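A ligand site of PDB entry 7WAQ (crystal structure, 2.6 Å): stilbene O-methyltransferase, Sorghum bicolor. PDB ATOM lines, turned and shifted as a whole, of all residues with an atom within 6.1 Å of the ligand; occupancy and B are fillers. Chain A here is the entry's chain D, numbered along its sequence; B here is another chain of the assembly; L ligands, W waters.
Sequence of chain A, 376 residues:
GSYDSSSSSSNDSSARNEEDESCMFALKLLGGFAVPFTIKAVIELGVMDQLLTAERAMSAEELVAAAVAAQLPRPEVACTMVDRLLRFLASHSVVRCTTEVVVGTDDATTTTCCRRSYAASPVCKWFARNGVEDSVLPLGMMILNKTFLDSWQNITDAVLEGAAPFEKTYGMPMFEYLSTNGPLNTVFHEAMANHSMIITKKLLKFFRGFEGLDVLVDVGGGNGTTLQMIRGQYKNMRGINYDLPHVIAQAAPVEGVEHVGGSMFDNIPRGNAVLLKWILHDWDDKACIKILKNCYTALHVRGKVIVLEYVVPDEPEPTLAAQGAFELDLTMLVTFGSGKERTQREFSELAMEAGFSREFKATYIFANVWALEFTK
Water W1 lies within hydrogen-bond range of an oxygen (O1) of the ligand (2.9 Å), the side-chain hydroxyl (OH) of Tyr 310 (3.1 Å) and the backbone carbonyl oxygen (O) of Gly 324 (3.5 Å).
ND1 of His 281 lies close to SD of Met 332. O of Thr 331 sits at hydrogen-bond distance from OG1 of Thr 335 (2.7 Å). NE2 of His 281 lies within hydrogen-bond range of O of Trp 278, at 3.4 Å. A ring nitrogen (NE2) of His 281 sits close to the side-chain carboxylate of Asp 282, 2.9 Å away.
A ring nitrogen (NE2) of His 281 lies within hydrogen-bond range of an oxygen (O3) of the ligand, 2.9 Å away. The side-chain carboxylate of Asp 282 lies within hydrogen-bond range of an oxygen (O3) of the ligand.
CE of Met 142 touches C7 of the ligand, 3.7 Å away. Ile 143 touches the ligand. Phe 148 touches the ligand. Met 174 touches the ligand. CE1 of Phe 188 touches O2 of the ligand (3.7 Å). CE of Met 192 touches C6 of the ligand (3.8 Å). Trp 278 touches the ligand. OH of Tyr 310 touches C13 of the ligand, at 3.5 Å. Leu 328 touches the ligand (CD1 to C8, 3.7 Å). Met 332 touches the ligand (CE to C3, 3.6 Å). Thr 335 touches the ligand (CG2 to O2, 3.3 Å). CB of Leu 27 of chain B touches O1 of the ligand, at 3.4 Å. Hydrophobic or aromatic side chains that line the ligand: Met 142, Ile 143, Phe 148, Met 174, Phe 188, Met 192, Trp 278, His 281, Leu 328, Met 332 and Leu 27 of chain B. The nearest printed residue that does not touch the ligand is Leu 139 (4.1 Å).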
ATOM      1  N   LEU A 139      15.746  -0.021  -8.677  1.00  0.00           N
ATOM      2  CA  LEU A 139      16.049   0.868  -9.784  1.00  0.00           C
ATOM      3  C   LEU A 139      17.275   0.362 -10.559  1.00  0.00           C
ATOM      4  O   LEU A 139      17.288   0.331 -11.782  1.00  0.00           O
ATOM      5  CB  LEU A 139      16.257   2.309  -9.260  1.00  0.00           C
ATOM      6  CG  LEU A 139      16.695   3.322 -10.352  1.00  0.00           C
ATOM      7  CD1 LEU A 139      15.737   3.382 -11.579  1.00  0.00           C
ATOM      8  CD2 LEU A 139      16.889   4.766  -9.811  1.00  0.00           C
ATOM      9  N   MET A 142      16.726  -2.507 -12.853  1.00  0.00           N
ATOM     10  CA  MET A 142      16.142  -2.102 -14.122  1.00  0.00           C
ATOM     11  C   MET A 142      17.210  -1.502 -15.050  1.00  0.00           C
ATOM     12  O   MET A 142      17.242  -1.825 -16.233  1.00  0.00           O
ATOM     13  CB  MET A 142      15.049  -1.037 -13.918  1.00  0.00           C
ATOM     14  CG  MET A 142      14.411  -0.642 -15.247  1.00  0.00           C
ATOM     15  SD  MET A 142      13.596   0.938 -15.285  1.00  0.00           S
ATOM     16  CE  MET A 142      14.865   2.127 -14.809  1.00  0.00           C
ATOM     17  N   ILE A 143      18.019  -0.579 -14.483  1.00  0.00           N
ATOM     18  CA  ILE A 143      19.119   0.024 -15.226  1.00  0.00           C
ATOM     19  C   ILE A 143      19.955  -1.062 -15.868  1.00  0.00           C
ATOM     20  O   ILE A 143      20.419  -0.835 -16.956  1.00  0.00           O
ATOM     21  CB  ILE A 143      19.962   0.929 -14.311  1.00  0.00           C
ATOM     22  CG1 ILE A 143      19.182   2.115 -13.773  1.00  0.00           C
ATOM     23  CG2 ILE A 143      21.225   1.427 -15.016  1.00  0.00           C
ATOM     24  CD1 ILE A 143      19.819   2.654 -12.456  1.00  0.00           C
ATOM     25  N   PHE A 148      16.998  -3.684 -21.559  1.00  0.00           N
ATOM     26  CA  PHE A 148      17.446  -2.336 -21.775  1.00  0.00           C
ATOM     27  C   PHE A 148      18.905  -2.280 -22.189  1.00  0.00           C
ATOM     28  O   PHE A 148      19.330  -1.416 -22.938  1.00  0.00           O
ATOM     29  CB  PHE A 148      17.334  -1.573 -20.470  1.00  0.00           C
ATOM     30  CG  PHE A 148      15.951  -1.114 -20.121  1.00  0.00           C
ATOM     31  CD1 PHE A 148      14.915  -2.001 -19.961  1.00  0.00           C
ATOM     32  CD2 PHE A 148      15.715   0.244 -19.936  1.00  0.00           C
ATOM     33  CE1 PHE A 148      13.655  -1.551 -19.636  1.00  0.00           C
ATOM     34  CE2 PHE A 148      14.461   0.704 -19.603  1.00  0.00           C
ATOM     35  CZ  PHE A 148      13.429  -0.209 -19.463  1.00  0.00           C
ATOM     36  N   MET A 174       8.524   0.701 -25.681  1.00  0.00           N
ATOM     37  CA  MET A 174       8.826   0.014 -24.442  1.00  0.00           C
ATOM     38  C   MET A 174       7.519  -0.208 -23.682  1.00  0.00           C
ATOM     39  O   MET A 174       7.344  -1.297 -23.098  1.00  0.00           O
ATOM     40  CB  MET A 174       9.839   0.839 -23.652  1.00  0.00           C
ATOM     41  CG  MET A 174      10.369   0.111 -22.458  1.00  0.00           C
ATOM     42  SD  MET A 174       9.412   0.526 -20.913  1.00  0.00           S
ATOM     43  CE  MET A 174       9.805   2.254 -20.652  1.00  0.00           C
ATOM     44  N   PHE A 188       9.932  -2.886 -13.969  1.00  0.00           N
ATOM     45  CA  PHE A 188       9.794  -1.493 -14.262  1.00  0.00           C
ATOM     46  C   PHE A 188       9.006  -0.840 -13.112  1.00  0.00           C
ATOM     47  O   PHE A 188       9.473   0.194 -12.552  1.00  0.00           O
ATOM     48  CB  PHE A 188       9.172  -1.309 -15.629  1.00  0.00           C
ATOM     49  CG  PHE A 188       9.010   0.159 -15.969  1.00  0.00           C
ATOM     50  CD1 PHE A 188      10.032   0.867 -16.558  1.00  0.00           C
ATOM     51  CD2 PHE A 188       7.840   0.841 -15.652  1.00  0.00           C
ATOM     52  CE1 PHE A 188       9.858   2.222 -16.890  1.00  0.00           C
ATOM     53  CE2 PHE A 188       7.694   2.209 -15.935  1.00  0.00           C
ATOM     54  CZ  PHE A 188       8.688   2.904 -16.573  1.00  0.00           C
ATOM     55  N   MET A 192      10.224   2.112 -10.464  1.00  0.00           N
ATOM     56  CA  MET A 192       9.601   3.426 -10.385  1.00  0.00           C
ATOM     57  C   MET A 192       9.074   3.649  -8.963  1.00  0.00           C
ATOM     58  O   MET A 192       9.156   4.766  -8.432  1.00  0.00           O
ATOM     59  CB  MET A 192       8.436   3.605 -11.379  1.00  0.00           C
ATOM     60  CG  MET A 192       8.776   3.564 -12.922  1.00  0.00           C
ATOM     61  SD  MET A 192       9.994   4.838 -13.455  1.00  0.00           S
ATOM     62  CE  MET A 192      11.408   3.772 -13.787  1.00  0.00           C
ATOM     63  N   HIS A 195      12.149   4.542  -6.799  1.00  0.00           N
ATOM     64  CA  HIS A 195      12.614   5.917  -6.954  1.00  0.00           C
ATOM     65  C   HIS A 195      11.592   6.849  -6.306  1.00  0.00           C
ATOM     66  O   HIS A 195      11.909   7.818  -5.609  1.00  0.00           O
ATOM     67  CB  HIS A 195      12.833   6.251  -8.448  1.00  0.00           C
ATOM     68  CG  HIS A 195      13.612   7.525  -8.634  1.00  0.00           C
ATOM     69  ND1 HIS A 195      13.033   8.716  -8.993  1.00  0.00           N
ATOM     70  CD2 HIS A 195      14.974   7.768  -8.531  1.00  0.00           C
ATOM     71  CE1 HIS A 195      13.981   9.687  -9.038  1.00  0.00           C
ATOM     72  NE2 HIS A 195      15.192   9.123  -8.710  1.00  0.00           N
ATOM     73  N   TRP A 278       8.495  12.338 -13.436  1.00  0.00           N
ATOM     74  CA  TRP A 278       9.148  11.503 -14.432  1.00  0.00           C
ATOM     75  C   TRP A 278       8.170  11.108 -15.502  1.00  0.00           C
ATOM     76  O   TRP A 278       8.214   9.962 -16.012  1.00  0.00           O
ATOM     77  CB  TRP A 278       9.809  10.255 -13.841  1.00  0.00           C
ATOM     78  CG  TRP A 278      11.270  10.417 -13.534  1.00  0.00           C
ATOM     79  CD1 TRP A 278      12.065  11.497 -13.792  1.00  0.00           C
ATOM     80  CD2 TRP A 278      12.138   9.402 -12.994  1.00  0.00           C
ATOM     81  NE1 TRP A 278      13.343  11.274 -13.359  1.00  0.00           N
ATOM     82  CE2 TRP A 278      13.425   9.987 -12.870  1.00  0.00           C
ATOM     83  CE3 TRP A 278      11.946   8.080 -12.543  1.00  0.00           C
ATOM     84  CZ2 TRP A 278      14.504   9.275 -12.345  1.00  0.00           C
ATOM     85  CZ3 TRP A 278      13.002   7.386 -12.011  1.00  0.00           C
ATOM     86  CH2 TRP A 278      14.272   7.979 -11.920  1.00  0.00           C
ATOM     87  N   ILE A 279       7.336  12.105 -15.869  1.00  0.00           N
ATOM     88  CA  ILE A 279       6.336  11.932 -16.920  1.00  0.00           C
ATOM     89  C   ILE A 279       6.878  12.634 -18.168  1.00  0.00           C
ATOM     90  O   ILE A 279       7.080  12.006 -19.232  1.00  0.00           O
ATOM     91  CB  ILE A 279       4.945  12.496 -16.533  1.00  0.00           C
ATOM     92  CG1 ILE A 279       4.366  12.019 -15.190  1.00  0.00           C
ATOM     93  CG2 ILE A 279       4.037  12.179 -17.690  1.00  0.00           C
ATOM     94  CD1 ILE A 279       4.271  10.491 -14.975  1.00  0.00           C
ATOM     95  N   HIS A 281       9.665  13.699 -19.095  1.00  0.00           N
ATOM     96  CA  HIS A 281      10.929  13.430 -19.710  1.00  0.00           C
ATOM     97  C   HIS A 281      10.793  12.251 -20.684  1.00  0.00           C
ATOM     98  O   HIS A 281      11.712  11.985 -21.415  1.00  0.00           O
ATOM     99  CB  HIS A 281      11.975  13.288 -18.599  1.00  0.00           C
ATOM    100  CG  HIS A 281      12.033  11.963 -17.911  1.00  0.00           C
ATOM    101  ND1 HIS A 281      13.185  11.361 -17.489  1.00  0.00           N
ATOM    102  CD2 HIS A 281      10.992  11.101 -17.694  1.00  0.00           C
ATOM    103  CE1 HIS A 281      12.843  10.200 -16.935  1.00  0.00           C
ATOM    104  NE2 HIS A 281      11.496  10.025 -17.033  1.00  0.00           N
ATOM    105  N   ASP A 282       9.626  11.609 -20.741  1.00  0.00           N
ATOM    106  CA  ASP A 282       9.387  10.443 -21.568  1.00  0.00           C
ATOM    107  C   ASP A 282       8.946  10.827 -22.990  1.00  0.00           C
ATOM    108  O   ASP A 282       8.914   9.970 -23.896  1.00  0.00           O
ATOM    109  CB  ASP A 282       8.278   9.593 -20.947  1.00  0.00           C
ATOM    110  CG  ASP A 282       8.587   8.858 -19.646  1.00  0.00           C
ATOM    111  OD1 ASP A 282       9.667   8.982 -19.001  1.00  0.00           O
ATOM    112  OD2 ASP A 282       7.782   8.072 -19.356  1.00  0.00           O
ATOM    113  N   TYR A 310      14.849  15.743 -13.296  1.00  0.00           N
ATOM    114  CA  TYR A 310      16.205  16.277 -13.380  1.00  0.00           C
ATOM    115  C   TYR A 310      16.177  17.537 -14.260  1.00  0.00           C
ATOM    116  O   TYR A 310      15.248  17.827 -14.963  1.00  0.00           O
ATOM    117  CB  TYR A 310      17.196  15.263 -13.960  1.00  0.00           C
ATOM    118  CG  TYR A 310      17.580  14.003 -13.220  1.00  0.00           C
ATOM    119  CD1 TYR A 310      16.711  13.351 -12.364  1.00  0.00           C
ATOM    120  CD2 TYR A 310      18.807  13.398 -13.499  1.00  0.00           C
ATOM    121  CE1 TYR A 310      17.052  12.104 -11.797  1.00  0.00           C
ATOM    122  CE2 TYR A 310      19.191  12.212 -12.868  1.00  0.00           C
ATOM    123  CZ  TYR A 310      18.308  11.565 -12.030  1.00  0.00           C
ATOM    124  OH  TYR A 310      18.689  10.405 -11.436  1.00  0.00           O
ATOM    125  N   GLY A 324      25.446  12.694 -14.550  1.00  0.00           N
ATOM    126  CA  GLY A 324      24.326  11.824 -14.216  1.00  0.00           C
ATOM    127  C   GLY A 324      23.069  12.241 -14.975  1.00  0.00           C
ATOM    128  O   GLY A 324      22.285  11.407 -15.403  1.00  0.00           O
ATOM    129  N   GLU A 327      23.463  11.345 -18.569  1.00  0.00           N
ATOM    130  CA  GLU A 327      23.266   9.904 -18.643  1.00  0.00           C
ATOM    131  C   GLU A 327      21.775   9.545 -18.658  1.00  0.00           C
ATOM    132  O   GLU A 327      21.351   8.595 -19.330  1.00  0.00           O
ATOM    133  CB  GLU A 327      23.917   9.245 -17.420  1.00  0.00           C
ATOM    134  CG  GLU A 327      24.202   7.792 -17.587  1.00  0.00           C
ATOM    135  CD  GLU A 327      24.480   6.901 -16.415  1.00  0.00           C
ATOM    136  OE1 GLU A 327      24.152   5.741 -16.735  1.00  0.00           O
ATOM    137  OE2 GLU A 327      24.978   7.359 -15.243  1.00  0.00           O
ATOM    138  N   LEU A 328      20.990  10.233 -17.807  1.00  0.00           N
ATOM    139  CA  LEU A 328      19.569  10.046 -17.818  1.00  0.00           C
ATOM    140  C   LEU A 328      19.020  10.452 -19.193  1.00  0.00           C
ATOM    141  O   LEU A 328      18.174   9.772 -19.756  1.00  0.00           O
ATOM    142  CB  LEU A 328      18.919  10.838 -16.693  1.00  0.00           C
ATOM    143  CG  LEU A 328      17.409  10.585 -16.641  1.00  0.00           C
ATOM    144  CD1 LEU A 328      17.109   9.100 -16.762  1.00  0.00           C
ATOM    145  CD2 LEU A 328      16.761  11.111 -15.368  1.00  0.00           C
ATOM    146  N   THR A 331      19.514   7.564 -21.448  1.00  0.00           N
ATOM    147  CA  THR A 331      18.527   6.523 -21.121  1.00  0.00           C
ATOM    148  C   THR A 331      17.179   6.840 -21.766  1.00  0.00           C
ATOM    149  O   THR A 331      16.529   5.984 -22.361  1.00  0.00           O
ATOM    150  CB  THR A 331      18.390   6.339 -19.607  1.00  0.00           C
ATOM    151  OG1 THR A 331      19.702   6.210 -19.036  1.00  0.00           O
ATOM    152  CG2 THR A 331      17.627   5.060 -19.365  1.00  0.00           C
ATOM    153  N   MET A 332      16.797   8.111 -21.726  1.00  0.00           N
ATOM    154  CA  MET A 332      15.543   8.484 -22.356  1.00  0.00           C
ATOM    155  C   MET A 332      15.702   8.317 -23.858  1.00  0.00           C
ATOM    156  O   MET A 332      14.867   7.714 -24.516  1.00  0.00           O
ATOM    157  CB  MET A 332      15.114   9.919 -21.993  1.00  0.00           C
ATOM    158  CG  MET A 332      14.759  10.153 -20.496  1.00  0.00           C
ATOM    159  SD  MET A 332      13.399   9.140 -20.074  1.00  0.00           S
ATOM    160  CE  MET A 332      14.222   7.655 -19.530  1.00  0.00           C
ATOM    161  N   THR A 335      15.515   4.516 -24.556  1.00  0.00           N
ATOM    162  CA  THR A 335      14.249   3.970 -24.143  1.00  0.00           C
ATOM    163  C   THR A 335      13.164   4.452 -25.078  1.00  0.00           C
ATOM    164  O   THR A 335      12.345   3.636 -25.469  1.00  0.00           O
ATOM    165  CB  THR A 335      13.872   4.368 -22.690  1.00  0.00           C
ATOM    166  OG1 THR A 335      14.830   3.956 -21.740  1.00  0.00           O
ATOM    167  CG2 THR A 335      12.634   3.684 -22.186  1.00  0.00           C
ATOM    168  N   PHE A 336      13.118   5.774 -25.340  1.00  0.00           N
ATOM    169  CA  PHE A 336      11.994   6.520 -25.932  1.00  0.00           C
ATOM    170  C   PHE A 336      12.319   7.265 -27.239  1.00  0.00           C
ATOM    171  O   PHE A 336      11.365   7.577 -27.985  1.00  0.00           O
ATOM    172  CB  PHE A 336      11.513   7.624 -24.983  1.00  0.00           C
ATOM    173  CG  PHE A 336      10.881   7.027 -23.759  1.00  0.00           C
ATOM    174  CD1 PHE A 336       9.800   6.118 -23.860  1.00  0.00           C
ATOM    175  CD2 PHE A 336      11.366   7.338 -22.528  1.00  0.00           C
ATOM    176  CE1 PHE A 336       9.256   5.496 -22.747  1.00  0.00           C
ATOM    177  CE2 PHE A 336      10.749   6.791 -21.384  1.00  0.00           C
ATOM    178  CZ  PHE A 336       9.683   5.898 -21.512  1.00  0.00           C
ATOM    179  N   LEU B  27      24.475   5.538  -8.272  1.00  0.00           N
ATOM    180  CA  LEU B  27      23.861   5.485  -9.608  1.00  0.00           C
ATOM    181  C   LEU B  27      24.947   5.555 -10.692  1.00  0.00           C
ATOM    182  O   LEU B  27      24.849   4.859 -11.702  1.00  0.00           O
ATOM    183  CB  LEU B  27      22.886   6.666  -9.788  1.00  0.00           C
ATOM    184  CG  LEU B  27      21.644   6.657  -8.906  1.00  0.00           C
ATOM    185  CD1 LEU B  27      20.807   7.881  -9.167  1.00  0.00           C
ATOM    186  CD2 LEU B  27      20.752   5.396  -9.044  1.00  0.00           C
ATOM    187  N   LYS B  28      25.974   6.435 -10.452  1.00  0.00           N
ATOM    188  CA  LYS B  28      27.141   6.451 -11.317  1.00  0.00           C
ATOM    189  C   LYS B  28      27.761   5.068 -11.526  1.00  0.00           C
ATOM    190  O   LYS B  28      28.014   4.639 -12.686  1.00  0.00           O
ATOM    191  CB  LYS B  28      28.156   7.385 -10.723  1.00  0.00           C
ATOM    192  CG  LYS B  28      29.381   7.571 -11.633  1.00  0.00           C
ATOM    193  CD  LYS B  28      30.375   8.557 -11.025  1.00  0.00           C
ATOM    194  CE  LYS B  28      31.773   8.318 -11.506  1.00  0.00           C
ATOM    195  NZ  LYS B  28      31.760   8.924 -12.842  1.00  0.00           N
ATOM    196  N   GLY B  31      25.772   2.767 -13.673  1.00  0.00           N
ATOM    197  CA  GLY B  31      25.513   3.033 -15.092  1.00  0.00           C
ATOM    198  C   GLY B  31      26.732   3.340 -15.983  1.00  0.00           C
ATOM    199  O   GLY B  31      26.571   3.841 -17.068  1.00  0.00           O
HETATM  200  C1  LIG L   1      11.843   6.514 -16.436  1.00  0.00           C
HETATM  201  C2  LIG L   1      11.645   5.601 -17.486  1.00  0.00           C
HETATM  202  C3  LIG L   1      12.681   4.776 -17.903  1.00  0.00           C
HETATM  203  C4  LIG L   1      13.862   4.854 -17.200  1.00  0.00           C
HETATM  204  C5  LIG L   1      14.058   5.751 -16.131  1.00  0.00           C
HETATM  205  C6  LIG L   1      13.041   6.602 -15.734  1.00  0.00           C
HETATM  206  C7  LIG L   1      15.405   5.717 -15.574  1.00  0.00           C
HETATM  207  C8  LIG L   1      15.924   6.403 -14.583  1.00  0.00           C
HETATM  208  C9  LIG L   1      17.337   6.304 -14.193  1.00  0.00           C
HETATM  209  C10 LIG L   1      18.285   5.469 -14.833  1.00  0.00           C
HETATM  210  C11 LIG L   1      19.618   5.552 -14.447  1.00  0.00           C
HETATM  211  C12 LIG L   1      20.027   6.393 -13.396  1.00  0.00           C
HETATM  212  C13 LIG L   1      19.079   7.190 -12.748  1.00  0.00           C
HETATM  213  C14 LIG L   1      17.741   7.116 -13.118  1.00  0.00           C
HETATM  214  O1  LIG L   1      21.282   6.485 -12.794  1.00  0.00           O
HETATM  215  O2  LIG L   1      12.593   3.822 -18.895  1.00  0.00           O
HETATM  216  O3  LIG L   1      10.738   7.338 -16.229  1.00  0.00           O
HETATM  217  O   HOH W   1      21.264   9.400 -12.739  1.00  0.00           O
